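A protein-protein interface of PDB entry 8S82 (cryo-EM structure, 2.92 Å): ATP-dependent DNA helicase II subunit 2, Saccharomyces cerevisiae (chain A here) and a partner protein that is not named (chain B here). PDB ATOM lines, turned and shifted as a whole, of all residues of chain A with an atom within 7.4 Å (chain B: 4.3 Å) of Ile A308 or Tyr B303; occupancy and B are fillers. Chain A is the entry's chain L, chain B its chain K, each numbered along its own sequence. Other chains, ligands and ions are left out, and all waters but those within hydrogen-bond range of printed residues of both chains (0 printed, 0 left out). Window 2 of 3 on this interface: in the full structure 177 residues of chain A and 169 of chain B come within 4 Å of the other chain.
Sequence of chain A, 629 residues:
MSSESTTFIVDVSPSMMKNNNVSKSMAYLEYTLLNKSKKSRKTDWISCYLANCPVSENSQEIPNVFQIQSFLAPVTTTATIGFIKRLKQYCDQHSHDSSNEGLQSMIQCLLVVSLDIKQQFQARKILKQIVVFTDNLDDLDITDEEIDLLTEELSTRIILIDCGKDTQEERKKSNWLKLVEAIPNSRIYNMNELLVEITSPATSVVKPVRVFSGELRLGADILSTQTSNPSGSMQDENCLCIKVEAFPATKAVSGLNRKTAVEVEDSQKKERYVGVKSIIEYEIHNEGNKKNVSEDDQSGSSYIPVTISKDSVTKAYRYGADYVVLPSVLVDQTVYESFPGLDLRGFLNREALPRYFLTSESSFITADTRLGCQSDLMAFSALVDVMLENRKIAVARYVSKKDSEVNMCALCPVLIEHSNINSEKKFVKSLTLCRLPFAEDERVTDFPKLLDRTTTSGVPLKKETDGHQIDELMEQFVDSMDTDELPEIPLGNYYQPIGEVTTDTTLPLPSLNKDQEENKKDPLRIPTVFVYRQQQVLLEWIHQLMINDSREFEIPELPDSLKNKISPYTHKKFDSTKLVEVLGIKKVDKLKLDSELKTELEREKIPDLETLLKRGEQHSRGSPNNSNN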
ATOM      1  N   ILE A 280       9.481 -14.179 -27.435  1.00  0.00           N
ATOM      2  CA  ILE A 280       9.162 -13.445 -26.217  1.00  0.00           C
ATOM      3  C   ILE A 280       7.878 -14.025 -25.641  1.00  0.00           C
ATOM      4  O   ILE A 280       6.896 -14.231 -26.363  1.00  0.00           O
ATOM      5  CB  ILE A 280       9.019 -11.937 -26.479  1.00  0.00           C
ATOM      6  CG1 ILE A 280       8.041 -11.675 -27.626  1.00  0.00           C
ATOM      7  CG2 ILE A 280      10.367 -11.321 -26.800  1.00  0.00           C
ATOM      8  CD1 ILE A 280       7.873 -10.209 -27.967  1.00  0.00           C
ATOM      9  N   GLU A 281       7.896 -14.305 -24.342  1.00  0.00           N
ATOM     10  CA  GLU A 281       6.740 -14.830 -23.637  1.00  0.00           C
ATOM     11  C   GLU A 281       6.488 -13.979 -22.404  1.00  0.00           C
ATOM     12  O   GLU A 281       7.399 -13.353 -21.858  1.00  0.00           O
ATOM     13  CB  GLU A 281       6.935 -16.296 -23.229  1.00  0.00           C
ATOM     14  CG  GLU A 281       7.139 -17.251 -24.390  1.00  0.00           C
ATOM     15  CD  GLU A 281       7.321 -18.683 -23.931  1.00  0.00           C
ATOM     16  OE1 GLU A 281       7.476 -18.900 -22.712  1.00  0.00           O
ATOM     17  OE2 GLU A 281       7.306 -19.592 -24.787  1.00  0.00           O
ATOM     18  N   TYR A 282       5.230 -13.945 -21.979  1.00  0.00           N
ATOM     19  CA  TYR A 282       4.829 -13.239 -20.771  1.00  0.00           C
ATOM     20  C   TYR A 282       4.243 -14.239 -19.790  1.00  0.00           C
ATOM     21  O   TYR A 282       3.323 -14.986 -20.136  1.00  0.00           O
ATOM     22  CB  TYR A 282       3.826 -12.131 -21.089  1.00  0.00           C
ATOM     23  CG  TYR A 282       4.432 -10.990 -21.871  1.00  0.00           C
ATOM     24  CD1 TYR A 282       5.123  -9.974 -21.226  1.00  0.00           C
ATOM     25  CD2 TYR A 282       4.321 -10.933 -23.252  1.00  0.00           C
ATOM     26  CE1 TYR A 282       5.682  -8.930 -21.935  1.00  0.00           C
ATOM     27  CE2 TYR A 282       4.879  -9.893 -23.970  1.00  0.00           C
ATOM     28  CZ  TYR A 282       5.557  -8.894 -23.306  1.00  0.00           C
ATOM     29  OH  TYR A 282       6.113  -7.856 -24.017  1.00  0.00           O
ATOM     30  N   GLU A 283       4.787 -14.264 -18.578  1.00  0.00           N
ATOM     31  CA  GLU A 283       4.364 -15.195 -17.543  1.00  0.00           C
ATOM     32  C   GLU A 283       4.050 -14.420 -16.271  1.00  0.00           C
ATOM     33  O   GLU A 283       4.682 -13.408 -15.960  1.00  0.00           O
ATOM     34  CB  GLU A 283       5.438 -16.256 -17.273  1.00  0.00           C
ATOM     35  CG  GLU A 283       5.755 -17.146 -18.462  1.00  0.00           C
ATOM     36  CD  GLU A 283       6.644 -18.317 -18.090  1.00  0.00           C
ATOM     37  OE1 GLU A 283       6.845 -18.547 -16.878  1.00  0.00           O
ATOM     38  OE2 GLU A 283       7.139 -19.005 -19.008  1.00  0.00           O
ATOM     39  N   ILE A 284       3.057 -14.907 -15.528  1.00  0.00           N
ATOM     40  CA  ILE A 284       2.679 -14.329 -14.245  1.00  0.00           C
ATOM     41  C   ILE A 284       2.800 -15.411 -13.182  1.00  0.00           C
ATOM     42  O   ILE A 284       2.827 -16.607 -13.476  1.00  0.00           O
ATOM     43  CB  ILE A 284       1.254 -13.731 -14.254  1.00  0.00           C
ATOM     44  CG1 ILE A 284       0.215 -14.768 -13.818  1.00  0.00           C
ATOM     45  CG2 ILE A 284       0.909 -13.196 -15.632  1.00  0.00           C
ATOM     46  CD1 ILE A 284      -0.215 -15.708 -14.915  1.00  0.00           C
ATOM     47  N   ASN A 286       1.033 -16.951  -9.990  1.00  0.00           N
ATOM     48  CA  ASN A 286      -0.173 -17.077  -9.173  1.00  0.00           C
ATOM     49  C   ASN A 286       0.245 -17.674  -7.835  1.00  0.00           C
ATOM     50  O   ASN A 286       1.015 -18.632  -7.768  1.00  0.00           O
ATOM     51  CB  ASN A 286      -1.219 -17.930  -9.880  1.00  0.00           C
ATOM     52  CG  ASN A 286      -2.637 -17.561  -9.484  1.00  0.00           C
ATOM     53  OD1 ASN A 286      -2.956 -17.463  -8.298  1.00  0.00           O
ATOM     54  ND2 ASN A 286      -3.498 -17.361 -10.476  1.00  0.00           N
ATOM     55  N   VAL A 306       2.442 -19.082 -14.937  1.00  0.00           N
ATOM     56  CA  VAL A 306       1.513 -19.363 -16.028  1.00  0.00           C
ATOM     57  C   VAL A 306       1.785 -18.371 -17.147  1.00  0.00           C
ATOM     58  O   VAL A 306       1.844 -17.161 -16.914  1.00  0.00           O
ATOM     59  CB  VAL A 306       0.039 -19.284 -15.577  1.00  0.00           C
ATOM     60  CG1 VAL A 306      -0.889 -19.399 -16.774  1.00  0.00           C
ATOM     61  CG2 VAL A 306      -0.270 -20.373 -14.558  1.00  0.00           C
ATOM     62  N   THR A 307       1.970 -18.888 -18.359  1.00  0.00           N
ATOM     63  CA  THR A 307       2.261 -18.050 -19.515  1.00  0.00           C
ATOM     64  C   THR A 307       0.967 -17.634 -20.209  1.00  0.00           C
ATOM     65  O   THR A 307       0.152 -18.483 -20.585  1.00  0.00           O
ATOM     66  CB  THR A 307       3.185 -18.785 -20.486  1.00  0.00           C
ATOM     67  OG1 THR A 307       3.154 -18.140 -21.765  1.00  0.00           O
ATOM     68  CG2 THR A 307       2.767 -20.244 -20.633  1.00  0.00           C
ATOM     69  N   ILE A 308       0.784 -16.328 -20.376  1.00  0.00           N
ATOM     70  CA  ILE A 308      -0.339 -15.776 -21.116  1.00  0.00           C
ATOM     71  C   ILE A 308       0.212 -14.858 -22.201  1.00  0.00           C
ATOM     72  O   ILE A 308       1.274 -14.245 -22.055  1.00  0.00           O
ATOM     73  CB  ILE A 308      -1.320 -15.021 -20.193  1.00  0.00           C
ATOM     74  CG1 ILE A 308      -1.687 -15.882 -18.984  1.00  0.00           C
ATOM     75  CG2 ILE A 308      -2.588 -14.633 -20.943  1.00  0.00           C
ATOM     76  CD1 ILE A 308      -2.471 -17.129 -19.336  1.00  0.00           C
ATOM     77  N   SER A 309      -0.524 -14.766 -23.305  1.00  0.00           N
ATOM     78  CA  SER A 309      -0.072 -13.978 -24.444  1.00  0.00           C
ATOM     79  C   SER A 309      -0.119 -12.489 -24.126  1.00  0.00           C
ATOM     80  O   SER A 309      -0.817 -12.044 -23.212  1.00  0.00           O
ATOM     81  CB  SER A 309      -0.927 -14.278 -25.674  1.00  0.00           C
ATOM     82  OG  SER A 309      -0.783 -15.631 -26.074  1.00  0.00           O
ATOM     83  N   LYS A 310       0.640 -11.716 -24.899  1.00  0.00           N
ATOM     84  CA  LYS A 310       0.766 -10.278 -24.704  1.00  0.00           C
ATOM     85  C   LYS A 310      -0.528  -9.521 -24.972  1.00  0.00           C
ATOM     86  O   LYS A 310      -0.633  -8.354 -24.582  1.00  0.00           O
ATOM     87  CB  LYS A 310       1.876  -9.719 -25.599  1.00  0.00           C
ATOM     88  CG  LYS A 310       1.544  -9.712 -27.081  1.00  0.00           C
ATOM     89  CD  LYS A 310       2.717  -9.203 -27.905  1.00  0.00           C
ATOM     90  CE  LYS A 310       3.171  -7.832 -27.434  1.00  0.00           C
ATOM     91  NZ  LYS A 310       2.065  -6.835 -27.473  1.00  0.00           N
ATOM     92  N   ASP A 311      -1.508 -10.144 -25.627  1.00  0.00           N
ATOM     93  CA  ASP A 311      -2.776  -9.468 -25.868  1.00  0.00           C
ATOM     94  C   ASP A 311      -3.580  -9.297 -24.586  1.00  0.00           C
ATOM     95  O   ASP A 311      -4.420  -8.394 -24.502  1.00  0.00           O
ATOM     96  CB  ASP A 311      -3.597 -10.240 -26.901  1.00  0.00           C
ATOM     97  CG  ASP A 311      -2.879 -10.381 -28.227  1.00  0.00           C
ATOM     98  OD1 ASP A 311      -1.791 -10.994 -28.253  1.00  0.00           O
ATOM     99  OD2 ASP A 311      -3.403  -9.882 -29.246  1.00  0.00           O
ATOM    100  N   SER A 312      -3.337 -10.142 -23.584  1.00  0.00           N
ATOM    101  CA  SER A 312      -4.007 -10.049 -22.295  1.00  0.00           C
ATOM    102  C   SER A 312      -3.163  -9.320 -21.255  1.00  0.00           C
ATOM    103  O   SER A 312      -3.538  -9.279 -20.077  1.00  0.00           O
ATOM    104  CB  SER A 312      -4.380 -11.444 -21.793  1.00  0.00           C
ATOM    105  OG  SER A 312      -5.199 -11.359 -20.641  1.00  0.00           O
ATOM    106  N   VAL A 313      -2.031  -8.755 -21.661  1.00  0.00           N
ATOM    107  CA  VAL A 313      -1.141  -8.015 -20.775  1.00  0.00           C
ATOM    108  C   VAL A 313      -1.158  -6.552 -21.196  1.00  0.00           C
ATOM    109  O   VAL A 313      -0.952  -6.235 -22.373  1.00  0.00           O
ATOM    110  CB  VAL A 313       0.288  -8.586 -20.808  1.00  0.00           C
ATOM    111  CG1 VAL A 313       1.260  -7.626 -20.149  1.00  0.00           C
ATOM    112  CG2 VAL A 313       0.327  -9.936 -20.116  1.00  0.00           C
ATOM    113  N   THR A 314      -1.406  -5.666 -20.234  1.00  0.00           N
ATOM    114  CA  THR A 314      -1.530  -4.242 -20.499  1.00  0.00           C
ATOM    115  C   THR A 314      -0.490  -3.487 -19.688  1.00  0.00           C
ATOM    116  O   THR A 314      -0.043  -3.950 -18.636  1.00  0.00           O
ATOM    117  CB  THR A 314      -2.935  -3.720 -20.162  1.00  0.00           C
ATOM    118  OG1 THR A 314      -3.229  -3.988 -18.785  1.00  0.00           O
ATOM    119  CG2 THR A 314      -3.978  -4.399 -21.036  1.00  0.00           C
ATOM    120  N   LEU B 301       4.080  -4.344 -16.405  1.00  0.00           N
ATOM    121  CA  LEU B 301       3.218  -5.252 -17.155  1.00  0.00           C
ATOM    122  C   LEU B 301       2.246  -5.894 -16.175  1.00  0.00           C
ATOM    123  O   LEU B 301       2.663  -6.606 -15.256  1.00  0.00           O
ATOM    124  CB  LEU B 301       4.035  -6.316 -17.884  1.00  0.00           C
ATOM    125  CG  LEU B 301       4.962  -5.893 -19.025  1.00  0.00           C
ATOM    126  CD1 LEU B 301       4.317  -4.818 -19.886  1.00  0.00           C
ATOM    127  CD2 LEU B 301       6.311  -5.440 -18.495  1.00  0.00           C
ATOM    128  N   VAL B 302       0.954  -5.640 -16.361  1.00  0.00           N
ATOM    129  CA  VAL B 302      -0.083  -6.175 -15.490  1.00  0.00           C
ATOM    130  C   VAL B 302      -1.022  -7.044 -16.313  1.00  0.00           C
ATOM    131  O   VAL B 302      -1.484  -6.639 -17.387  1.00  0.00           O
ATOM    132  CB  VAL B 302      -0.853  -5.060 -14.764  1.00  0.00           C
ATOM    133  CG1 VAL B 302      -0.008  -4.485 -13.645  1.00  0.00           C
ATOM    134  CG2 VAL B 302      -1.251  -3.975 -15.734  1.00  0.00           C
ATOM    135  N   TYR B 303      -1.287  -8.239 -15.806  1.00  0.00           N
ATOM    136  CA  TYR B 303      -2.258  -9.162 -16.368  1.00  0.00           C
ATOM    137  C   TYR B 303      -3.550  -9.031 -15.573  1.00  0.00           C
ATOM    138  O   TYR B 303      -3.542  -9.139 -14.341  1.00  0.00           O
ATOM    139  CB  TYR B 303      -1.715 -10.590 -16.321  1.00  0.00           C
ATOM    140  CG  TYR B 303      -2.718 -11.676 -16.637  1.00  0.00           C
ATOM    141  CD1 TYR B 303      -3.163 -12.541 -15.647  1.00  0.00           C
ATOM    142  CD2 TYR B 303      -3.208 -11.845 -17.923  1.00  0.00           C
ATOM    143  CE1 TYR B 303      -4.073 -13.539 -15.928  1.00  0.00           C
ATOM    144  CE2 TYR B 303      -4.118 -12.842 -18.214  1.00  0.00           C
ATOM    145  CZ  TYR B 303      -4.548 -13.685 -17.213  1.00  0.00           C
ATOM    146  OH  TYR B 303      -5.456 -14.678 -17.499  1.00  0.00           O
ATOM    147  N   GLU B 304      -4.649  -8.772 -16.277  1.00  0.00           N
ATOM    148  CA  GLU B 304      -5.963  -8.582 -15.671  1.00  0.00           C
ATOM    149  C   GLU B 304      -6.857  -9.735 -16.100  1.00  0.00           C
ATOM    150  O   GLU B 304      -7.008  -9.995 -17.300  1.00  0.00           O
ATOM    151  CB  GLU B 304      -6.564  -7.240 -16.085  1.00  0.00           C
ATOM    152  CG  GLU B 304      -8.054  -7.105 -15.812  1.00  0.00           C
ATOM    153  CD  GLU B 304      -8.365  -6.839 -14.353  1.00  0.00           C
ATOM    154  OE1 GLU B 304      -7.417  -6.623 -13.571  1.00  0.00           O
ATOM    155  OE2 GLU B 304      -9.559  -6.842 -13.988  1.00  0.00           O
ATOM    156  N   HIS B 305      -7.447 -10.426 -15.127  1.00  0.00           N
ATOM    157  CA  HIS B 305      -8.362 -11.532 -15.388  1.00  0.00           C
ATOM    158  C   HIS B 305      -9.625 -11.305 -14.570  1.00  0.00           C
ATOM    159  O   HIS B 305      -9.570 -11.256 -13.336  1.00  0.00           O
ATOM    160  CB  HIS B 305      -7.719 -12.882 -15.058  1.00  0.00           C
ATOM    161  CG  HIS B 305      -7.108 -12.950 -13.694  1.00  0.00           C
ATOM    162  ND1 HIS B 305      -5.969 -12.251 -13.352  1.00  0.00           N
ATOM    163  CD2 HIS B 305      -7.467 -13.646 -12.590  1.00  0.00           C
ATOM    164  CE1 HIS B 305      -5.659 -12.508 -12.095  1.00  0.00           C
ATOM    165  NE2 HIS B 305      -6.551 -13.353 -11.610  1.00  0.00           N
ATOM    166  N   ILE B 308      -9.328  -9.269 -11.237  1.00  0.00           N
ATOM    167  CA  ILE B 308      -8.107  -9.437 -10.457  1.00  0.00           C
ATOM    168  C   ILE B 308      -6.933  -9.011 -11.328  1.00  0.00           C
ATOM    169  O   ILE B 308      -6.760  -9.517 -12.445  1.00  0.00           O
ATOM    170  CB  ILE B 308      -7.935 -10.880  -9.966  1.00  0.00           C
ATOM    171  CG1 ILE B 308      -9.205 -11.358  -9.261  1.00  0.00           C
ATOM    172  CG2 ILE B 308      -6.735 -10.986  -9.036  1.00  0.00           C
ATOM    173  CD1 ILE B 308      -9.176 -12.820  -8.876  1.00  0.00           C
ATOM    174  N   ARG B 309      -6.123  -8.085 -10.819  1.00  0.00           N
ATOM    175  CA  ARG B 309      -4.969  -7.557 -11.533  1.00  0.00           C
ATOM    176  C   ARG B 309      -3.701  -8.001 -10.821  1.00  0.00           C
ATOM    177  O   ARG B 309      -3.604  -7.889  -9.595  1.00  0.00           O
ATOM    178  CB  ARG B 309      -5.026  -6.028 -11.617  1.00  0.00           C
ATOM    179  CG  ARG B 309      -3.943  -5.406 -12.481  1.00  0.00           C
ATOM    180  CD  ARG B 309      -4.218  -3.932 -12.732  1.00  0.00           C
ATOM    181  NE  ARG B 309      -4.155  -3.144 -11.508  1.00  0.00           N
ATOM    182  CZ  ARG B 309      -3.086  -2.474 -11.102  1.00  0.00           C
ATOM    183  NH1 ARG B 309      -1.966  -2.468 -11.804  1.00  0.00           N
ATOM    184  NH2 ARG B 309      -3.142  -1.793  -9.962  1.00  0.00           N
ATOM    185  N   GLN B 310      -2.735  -8.505 -11.586  1.00  0.00           N
ATOM    186  CA  GLN B 310      -1.472  -8.959 -11.019  1.00  0.00           C
ATOM    187  C   GLN B 310      -0.351  -8.473 -11.926  1.00  0.00           C
ATOM    188  O   GLN B 310      -0.584  -8.085 -13.067  1.00  0.00           O
ATOM    189  CB  GLN B 310      -1.459 -10.485 -10.862  1.00  0.00           C
ATOM    190  CG  GLN B 310      -0.269 -11.042 -10.099  1.00  0.00           C
ATOM    191  CD  GLN B 310      -0.056 -10.355  -8.763  1.00  0.00           C
ATOM    192  OE1 GLN B 310       1.070 -10.011  -8.406  1.00  0.00           O
ATOM    193  NE2 GLN B 310      -1.136 -10.161  -8.016  1.00  0.00           N
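The backbone NH (N) of Val B302 lies within hydrogen-bond range of the backbone carbonyl oxygen (O) of Thr A314 (3.0 Å).
The backbone NH (N) of Val A306 lies within hydrogen-bond range of the backbone carbonyl oxygen (O) of Ile A284, at 2.9 Å.
The backbone NH (N) of Tyr B303 is in hydrogen-bond range of the backbone carbonyl oxygen (O) of Gln B310 (2.8 Å).
N of Ile A308 is in hydrogen-bond range of O of Tyr A282 (2.9 Å).
OE1 of Glu B304 lies close to N of Arg B309 (3.4 Å).
Among the printed residues, pairs that only touch across the chains: Ser A312 with Tyr B303, Ile A308 with Tyr B303, Val A313 with Val B302, Ile A284 with Tyr B303, Thr A314 with Leu B301, Val A313 with Leu B301 and Ser A312 with Glu B304.
Printed residues of chain B within 4 Å of Ile A284: Tyr B303.
Ile A308 touches just one residue of chain B: Tyr B303 (3.6 Å).
Asp A311 touches none of the printed residues of chain B.
Printed residues of chain B within 4 Å of Ser A312: Tyr B303 (3.0 Å) and Glu B304 (3.99 Å).
Printed residues of chain A within 4 Å of Leu B301: Val A313 and Thr A314.
Of the printed residues of chain A, Val B302 touches Val A313 and Thr A314.
Tyr B303 touches just these residues of chain A: Ile A284, Ile A308 and Ser A312.
Of the printed residues of chain A, Glu B304 touches Ser A312 (3.99 Å).
The nearest printed residue of chain B that does not touch Ile A308 is Glu B304 (7.4 Å).
Hydrophobic or aromatic side chains of chain B that line the printed part of chain A: Leu B301, Val B302 and Tyr B303.
Hydrophobic or aromatic side chains of chain A within 4 Å of the printed part of chain B: Ile A284, Ile A308 and Val A313.
Among the printed residues, 8 pairs touch across the chains.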
